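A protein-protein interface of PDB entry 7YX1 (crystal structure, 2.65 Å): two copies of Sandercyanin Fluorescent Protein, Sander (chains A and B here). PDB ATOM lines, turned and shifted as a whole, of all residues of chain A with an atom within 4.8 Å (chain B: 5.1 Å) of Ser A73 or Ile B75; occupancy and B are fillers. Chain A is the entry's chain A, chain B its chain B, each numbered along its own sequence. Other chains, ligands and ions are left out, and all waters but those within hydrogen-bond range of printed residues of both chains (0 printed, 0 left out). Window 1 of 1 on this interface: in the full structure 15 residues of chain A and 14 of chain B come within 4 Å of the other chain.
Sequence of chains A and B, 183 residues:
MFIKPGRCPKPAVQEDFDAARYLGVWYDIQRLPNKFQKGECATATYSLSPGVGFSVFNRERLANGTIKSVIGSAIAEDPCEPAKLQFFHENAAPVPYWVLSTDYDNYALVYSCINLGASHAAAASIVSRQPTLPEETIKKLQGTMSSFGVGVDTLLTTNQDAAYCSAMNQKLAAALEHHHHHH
The side-chain hydroxyl (OG) of Ser A73 is in hydrogen-bond range of the backbone NH (N) of Val B52, at 2.9 Å.
The backbone carbonyl oxygen (O) of Gly A72 is in hydrogen-bond range of the backbone NH (N) of Val A56 (2.7 Å).
The backbone carbonyl oxygen (O) of Ser A73 sits at hydrogen-bond distance from the backbone NH (N) of Phe A88 (2.7 Å).
O of Ile A75 sits at hydrogen-bond distance from N of Gln A86, at 2.7 Å.
The backbone carbonyl oxygen (O) of Val B52 lies within hydrogen-bond range of the side-chain hydroxyl (OG) of Ser B49, at 3.3 Å.
O of Ser B73 lies within hydrogen-bond range of N of Phe B88 (2.8 Å).
The backbone carbonyl oxygen of Ile B75 sits at hydrogen-bond distance from the backbone NH of Gln B86 (2.7 Å).
O of Gly B51 touches CD1 of Ile A71, at 3.4 Å.
Ile A71 touches Val B52 (O to CG1, 3.9 Å).
O of Gly A72 touches CA of Gly B51, 3.4 Å away.
Gly A72 touches Val B52.
CB of Ser A73 touches CD1 of Ile B75, 3.6 Å away.
Ile B75 touches Ile A75 (CD1 to CD1, 3.5 Å).
Ile A75 touches Phe B88.
O of Phe A88 touches CG1 of Val B52, at 3.2 Å.
Ile B75 touches Phe A88.
Glu B77 touches Phe A88 (OE2 to CE2, 3.4 Å).
Ser A73 touches three residues of chain B.
Of the printed residues of chain A, Ile B75 touches Ser A73, Ile A75 and Phe A88.
Of the printed residues of chain B, Gly A72 touches Gly B51 (3.4 Å) and Val B52 (3.5 Å).
Of the printed residues of chain A, Gly B51 touches Ile A71, Gly A72 and Ser A73.
Of the printed residues of chain B, Phe A88 touches Val B52, Ile B75, Glu B77 and Phe B88.
Of the printed residues of chain B, Ile A71 touches Gly B51 and Val B52.
Of the printed residues of chain A, Glu B77 touches Phe A88.
Lys B84 touches none of the printed residues of chain A.
Ser B49 touches none of the printed residues of chain A.
The nearest residue of chain B that does not touch Ser A73 is Ser B49 (4.9 Å).
Of the 11 printed residues of chain A, 5 touch a printed residue of chain B.
Among the printed residues, 13 pairs touch across the chains.
Ser A73 touches Ile B75, but with the chains exchanged Ile A75 does not touch Ser B73 (4.6 Å).
Ile B75 touches its own counterpart, Ile A75.
Ile A75 touches Phe B88, and with the chains exchanged Phe A88 touches Ile B75.
Phe A88 touches its own counterpart, Phe B88.
Of the 13 pairs that touch across the chains among the printed residues, 4 have their exchanged pair printed and touching as well.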
ATOM      1  N   PHE A  54      -6.265 -15.442  18.593  1.00  0.00           N
ATOM      2  CA  PHE A  54      -7.106 -16.482  18.022  1.00  0.00           C
ATOM      3  C   PHE A  54      -6.400 -17.828  18.110  1.00  0.00           C
ATOM      4  O   PHE A  54      -5.198 -17.910  18.374  1.00  0.00           O
ATOM      5  CB  PHE A  54      -7.489 -16.170  16.565  1.00  0.00           C
ATOM      6  CG  PHE A  54      -6.318 -15.930  15.655  1.00  0.00           C
ATOM      7  CD1 PHE A  54      -5.745 -16.975  14.945  1.00  0.00           C
ATOM      8  CD2 PHE A  54      -5.805 -14.656  15.492  1.00  0.00           C
ATOM      9  CE1 PHE A  54      -4.677 -16.750  14.101  1.00  0.00           C
ATOM     10  CE2 PHE A  54      -4.737 -14.426  14.652  1.00  0.00           C
ATOM     11  CZ  PHE A  54      -4.172 -15.474  13.954  1.00  0.00           C
ATOM     12  N   SER A  55      -7.173 -18.887  17.892  1.00  0.00           N
ATOM     13  CA  SER A  55      -6.665 -20.248  17.949  1.00  0.00           C
ATOM     14  C   SER A  55      -6.146 -20.684  16.582  1.00  0.00           C
ATOM     15  O   SER A  55      -6.424 -20.063  15.554  1.00  0.00           O
ATOM     16  CB  SER A  55      -7.753 -21.209  18.430  1.00  0.00           C
ATOM     17  OG  SER A  55      -8.533 -21.679  17.343  1.00  0.00           O
ATOM     18  N   VAL A  56      -5.329 -21.734  16.606  1.00  0.00           N
ATOM     19  CA  VAL A  56      -4.676 -22.238  15.371  1.00  0.00           C
ATOM     20  C   VAL A  56      -4.828 -23.757  15.301  1.00  0.00           C
ATOM     21  O   VAL A  56      -4.541 -24.424  16.287  1.00  0.00           O
ATOM     22  CB  VAL A  56      -3.197 -21.794  15.314  1.00  0.00           C
ATOM     23  CG1 VAL A  56      -2.466 -22.408  14.132  1.00  0.00           C
ATOM     24  CG2 VAL A  56      -3.036 -20.283  15.334  1.00  0.00           C
ATOM     25  N   ILE A  71      -2.228 -28.152  17.111  1.00  0.00           N
ATOM     26  CA  ILE A  71      -3.053 -27.029  17.633  1.00  0.00           C
ATOM     27  C   ILE A  71      -2.082 -25.963  18.118  1.00  0.00           C
ATOM     28  O   ILE A  71      -0.928 -26.288  18.384  1.00  0.00           O
ATOM     29  CB  ILE A  71      -4.036 -27.461  18.744  1.00  0.00           C
ATOM     30  CG1 ILE A  71      -3.341 -28.234  19.866  1.00  0.00           C
ATOM     31  CG2 ILE A  71      -5.204 -28.235  18.165  1.00  0.00           C
ATOM     32  CD1 ILE A  71      -3.175 -27.436  21.135  1.00  0.00           C
ATOM     33  N   GLY A  72      -2.550 -24.734  18.197  1.00  0.00           N
ATOM     34  CA  GLY A  72      -1.668 -23.655  18.604  1.00  0.00           C
ATOM     35  C   GLY A  72      -2.464 -22.406  18.900  1.00  0.00           C
ATOM     36  O   GLY A  72      -3.678 -22.349  18.689  1.00  0.00           O
ATOM     37  N   SER A  73      -1.751 -21.397  19.397  1.00  0.00           N
ATOM     38  CA  SER A  73      -2.347 -20.121  19.761  1.00  0.00           C
ATOM     39  C   SER A  73      -1.559 -18.984  19.128  1.00  0.00           C
ATOM     40  O   SER A  73      -0.331 -19.053  19.016  1.00  0.00           O
ATOM     41  CB  SER A  73      -2.398 -19.945  21.280  1.00  0.00           C
ATOM     42  OG  SER A  73      -3.469 -20.683  21.837  1.00  0.00           O
ATOM     43  N   ALA A  74      -2.273 -17.937  18.725  1.00  0.00           N
ATOM     44  CA  ALA A  74      -1.693 -16.805  18.017  1.00  0.00           C
ATOM     45  C   ALA A  74      -2.005 -15.520  18.768  1.00  0.00           C
ATOM     46  O   ALA A  74      -3.173 -15.230  19.046  1.00  0.00           O
ATOM     47  CB  ALA A  74      -2.236 -16.724  16.593  1.00  0.00           C
ATOM     48  N   ILE A  75      -0.967 -14.751  19.087  1.00  0.00           N
ATOM     49  CA  ILE A  75      -1.116 -13.487  19.800  1.00  0.00           C
ATOM     50  C   ILE A  75      -0.209 -12.448  19.157  1.00  0.00           C
ATOM     51  O   ILE A  75       0.930 -12.747  18.783  1.00  0.00           O
ATOM     52  CB  ILE A  75      -0.795 -13.635  21.303  1.00  0.00           C
ATOM     53  CG1 ILE A  75      -1.836 -14.515  21.996  1.00  0.00           C
ATOM     54  CG2 ILE A  75      -0.718 -12.276  21.987  1.00  0.00           C
ATOM     55  CD1 ILE A  75      -1.249 -15.731  22.652  1.00  0.00           C
ATOM     56  N   GLN A  86       2.809 -13.736  17.054  1.00  0.00           N
ATOM     57  CA  GLN A  86       3.621 -14.811  17.604  1.00  0.00           C
ATOM     58  C   GLN A  86       2.749 -16.051  17.723  1.00  0.00           C
ATOM     59  O   GLN A  86       1.696 -16.012  18.368  1.00  0.00           O
ATOM     60  CB  GLN A  86       4.201 -14.429  18.969  1.00  0.00           C
ATOM     61  CG  GLN A  86       5.503 -15.132  19.319  1.00  0.00           C
ATOM     62  CD  GLN A  86       6.702 -14.480  18.663  1.00  0.00           C
ATOM     63  OE1 GLN A  86       6.584 -13.418  18.053  1.00  0.00           O
ATOM     64  NE2 GLN A  86       7.865 -15.109  18.789  1.00  0.00           N
ATOM     65  N   PHE A  87       3.180 -17.140  17.094  1.00  0.00           N
ATOM     66  CA  PHE A  87       2.431 -18.390  17.070  1.00  0.00           C
ATOM     67  C   PHE A  87       3.055 -19.377  18.044  1.00  0.00           C
ATOM     68  O   PHE A  87       4.257 -19.653  17.969  1.00  0.00           O
ATOM     69  CB  PHE A  87       2.408 -18.990  15.662  1.00  0.00           C
ATOM     70  CG  PHE A  87       1.281 -18.492  14.811  1.00  0.00           C
ATOM     71  CD1 PHE A  87       0.928 -17.155  14.832  1.00  0.00           C
ATOM     72  CD2 PHE A  87       0.580 -19.354  13.986  1.00  0.00           C
ATOM     73  CE1 PHE A  87      -0.098 -16.684  14.044  1.00  0.00           C
ATOM     74  CE2 PHE A  87      -0.455 -18.888  13.198  1.00  0.00           C
ATOM     75  CZ  PHE A  87      -0.794 -17.551  13.228  1.00  0.00           C
ATOM     76  N   PHE A  88       2.214 -19.874  18.942  1.00  0.00           N
ATOM     77  CA  PHE A  88       2.647 -20.834  19.974  1.00  0.00           C
ATOM     78  C   PHE A  88       2.000 -22.177  19.661  1.00  0.00           C
ATOM     79  O   PHE A  88       0.831 -22.378  19.957  1.00  0.00           O
ATOM     80  CB  PHE A  88       2.276 -20.306  21.360  1.00  0.00           C
ATOM     81  CG  PHE A  88       2.635 -18.866  21.627  1.00  0.00           C
ATOM     82  CD1 PHE A  88       1.807 -17.840  21.210  1.00  0.00           C
ATOM     83  CD2 PHE A  88       3.792 -18.538  22.311  1.00  0.00           C
ATOM     84  CE1 PHE A  88       2.135 -16.518  21.457  1.00  0.00           C
ATOM     85  CE2 PHE A  88       4.117 -17.215  22.558  1.00  0.00           C
ATOM     86  CZ  PHE A  88       3.289 -16.208  22.131  1.00  0.00           C
ATOM     87  N   SER B  49      -8.940 -23.368  26.717  1.00  0.00           N
ATOM     88  CA  SER B  49      -8.641 -22.631  25.473  1.00  0.00           C
ATOM     89  C   SER B  49      -8.619 -23.634  24.327  1.00  0.00           C
ATOM     90  O   SER B  49      -8.135 -24.745  24.528  1.00  0.00           O
ATOM     91  CB  SER B  49      -7.340 -21.913  25.613  1.00  0.00           C
ATOM     92  OG  SER B  49      -6.262 -22.764  25.273  1.00  0.00           O
ATOM     93  N   GLY B  51      -6.794 -23.519  21.696  1.00  0.00           N
ATOM     94  CA  GLY B  51      -5.413 -23.773  21.280  1.00  0.00           C
ATOM     95  C   GLY B  51      -4.505 -24.195  22.412  1.00  0.00           C
ATOM     96  O   GLY B  51      -4.819 -25.160  23.107  1.00  0.00           O
ATOM     97  N   VAL B  52      -3.383 -23.508  22.543  1.00  0.00           N
ATOM     98  CA  VAL B  52      -2.404 -23.869  23.596  1.00  0.00           C
ATOM     99  C   VAL B  52      -2.699 -23.044  24.844  1.00  0.00           C
ATOM    100  O   VAL B  52      -3.086 -21.881  24.728  1.00  0.00           O
ATOM    101  CB  VAL B  52      -0.937 -23.743  23.121  1.00  0.00           C
ATOM    102  CG1 VAL B  52      -0.685 -24.504  21.834  1.00  0.00           C
ATOM    103  CG2 VAL B  52      -0.466 -22.306  23.017  1.00  0.00           C
ATOM    104  N   GLY B  53      -2.625 -23.688  25.984  1.00  0.00           N
ATOM    105  CA  GLY B  53      -2.764 -22.941  27.242  1.00  0.00           C
ATOM    106  C   GLY B  53      -4.166 -22.747  27.757  1.00  0.00           C
ATOM    107  O   GLY B  53      -5.066 -23.451  27.310  1.00  0.00           O
ATOM    108  N   SER B  73      -4.884 -14.400  27.992  1.00  0.00           N
ATOM    109  CA  SER B  73      -4.471 -15.735  27.587  1.00  0.00           C
ATOM    110  C   SER B  73      -3.170 -16.097  28.286  1.00  0.00           C
ATOM    111  O   SER B  73      -2.266 -15.265  28.412  1.00  0.00           O
ATOM    112  CB  SER B  73      -4.297 -15.826  26.068  1.00  0.00           C
ATOM    113  OG  SER B  73      -5.554 -15.839  25.412  1.00  0.00           O
ATOM    114  N   ALA B  74      -3.080 -17.346  28.734  1.00  0.00           N
ATOM    115  CA  ALA B  74      -1.933 -17.848  29.477  1.00  0.00           C
ATOM    116  C   ALA B  74      -1.271 -18.960  28.679  1.00  0.00           C
ATOM    117  O   ALA B  74      -1.943 -19.908  28.260  1.00  0.00           O
ATOM    118  CB  ALA B  74      -2.357 -18.364  30.847  1.00  0.00           C
ATOM    119  N   ILE B  75       0.039 -18.848  28.474  1.00  0.00           N
ATOM    120  CA  ILE B  75       0.778 -19.784  27.634  1.00  0.00           C
ATOM    121  C   ILE B  75       2.137 -20.060  28.261  1.00  0.00           C
ATOM    122  O   ILE B  75       2.858 -19.129  28.631  1.00  0.00           O
ATOM    123  CB  ILE B  75       0.948 -19.251  26.197  1.00  0.00           C
ATOM    124  CG1 ILE B  75      -0.387 -19.288  25.451  1.00  0.00           C
ATOM    125  CG2 ILE B  75       2.008 -20.041  25.442  1.00  0.00           C
ATOM    126  CD1 ILE B  75      -0.286 -18.842  24.019  1.00  0.00           C
ATOM    127  N   ALA B  76       2.481 -21.342  28.379  1.00  0.00           N
ATOM    128  CA  ALA B  76       3.819 -21.764  28.792  1.00  0.00           C
ATOM    129  C   ALA B  76       4.681 -21.835  27.539  1.00  0.00           C
ATOM    130  O   ALA B  76       4.575 -22.776  26.750  1.00  0.00           O
ATOM    131  CB  ALA B  76       3.768 -23.102  29.519  1.00  0.00           C
ATOM    132  N   GLU B  77       5.541 -20.830  27.354  1.00  0.00           N
ATOM    133  CA  GLU B  77       6.316 -20.735  26.122  1.00  0.00           C
ATOM    134  C   GLU B  77       7.303 -21.888  25.980  1.00  0.00           C
ATOM    135  O   GLU B  77       7.659 -22.261  24.856  1.00  0.00           O
ATOM    136  CB  GLU B  77       7.041 -19.391  26.067  1.00  0.00           C
ATOM    137  CG  GLU B  77       6.097 -18.198  25.992  1.00  0.00           C
ATOM    138  CD  GLU B  77       6.739 -16.978  25.365  1.00  0.00           C
ATOM    139  OE1 GLU B  77       7.966 -17.006  25.122  1.00  0.00           O
ATOM    140  OE2 GLU B  77       6.019 -15.985  25.121  1.00  0.00           O
ATOM    141  N   LYS B  84       6.236 -22.067  34.337  1.00  0.00           N
ATOM    142  CA  LYS B  84       6.718 -20.727  34.003  1.00  0.00           C
ATOM    143  C   LYS B  84       5.921 -20.243  32.797  1.00  0.00           C
ATOM    144  O   LYS B  84       6.322 -20.422  31.647  1.00  0.00           O
ATOM    145  CB  LYS B  84       8.217 -20.737  33.729  1.00  0.00           C
ATOM    146  CG  LYS B  84       9.045 -21.261  34.886  1.00  0.00           C
ATOM    147  CD  LYS B  84      10.489 -21.484  34.479  1.00  0.00           C
ATOM    148  CE  LYS B  84      11.401 -21.475  35.691  1.00  0.00           C
ATOM    149  NZ  LYS B  84      12.836 -21.417  35.303  1.00  0.00           N
ATOM    150  N   LEU B  85       4.776 -19.627  33.070  1.00  0.00           N
ATOM    151  CA  LEU B  85       3.847 -19.198  32.040  1.00  0.00           C
ATOM    152  C   LEU B  85       4.027 -17.719  31.725  1.00  0.00           C
ATOM    153  O   LEU B  85       4.596 -16.954  32.508  1.00  0.00           O
ATOM    154  CB  LEU B  85       2.404 -19.460  32.475  1.00  0.00           C
ATOM    155  CG  LEU B  85       1.993 -20.922  32.636  1.00  0.00           C
ATOM    156  CD1 LEU B  85       1.310 -21.122  33.977  1.00  0.00           C
ATOM    157  CD2 LEU B  85       1.087 -21.347  31.492  1.00  0.00           C
ATOM    158  N   GLN B  86       3.530 -17.327  30.557  1.00  0.00           N
ATOM    159  CA  GLN B  86       3.445 -15.930  30.156  1.00  0.00           C
ATOM    160  C   GLN B  86       1.978 -15.555  30.006  1.00  0.00           C
ATOM    161  O   GLN B  86       1.205 -16.294  29.388  1.00  0.00           O
ATOM    162  CB  GLN B  86       4.198 -15.679  28.846  1.00  0.00           C
ATOM    163  CG  GLN B  86       4.533 -14.213  28.575  1.00  0.00           C
ATOM    164  CD  GLN B  86       5.603 -13.660  29.499  1.00  0.00           C
ATOM    165  OE1 GLN B  86       6.164 -14.380  30.325  1.00  0.00           O
ATOM    166  NE2 GLN B  86       5.893 -12.371  29.360  1.00  0.00           N
ATOM    167  N   PHE B  88      -0.810 -12.934  28.667  1.00  0.00           N
ATOM    168  CA  PHE B  88      -1.075 -11.876  27.676  1.00  0.00           C
ATOM    169  C   PHE B  88      -2.442 -11.282  27.986  1.00  0.00           C
ATOM    170  O   PHE B  88      -3.446 -11.756  27.465  1.00  0.00           O
ATOM    171  CB  PHE B  88      -0.942 -12.445  26.260  1.00  0.00           C
ATOM    172  CG  PHE B  88       0.224 -13.371  26.041  1.00  0.00           C
ATOM    173  CD1 PHE B  88       1.452 -12.878  25.640  1.00  0.00           C
ATOM    174  CD2 PHE B  88       0.092 -14.736  26.227  1.00  0.00           C
ATOM    175  CE1 PHE B  88       2.526 -13.728  25.439  1.00  0.00           C
ATOM    176  CE2 PHE B  88       1.165 -15.585  26.025  1.00  0.00           C
ATOM    177  CZ  PHE B  88       2.380 -15.080  25.628  1.00  0.00           C
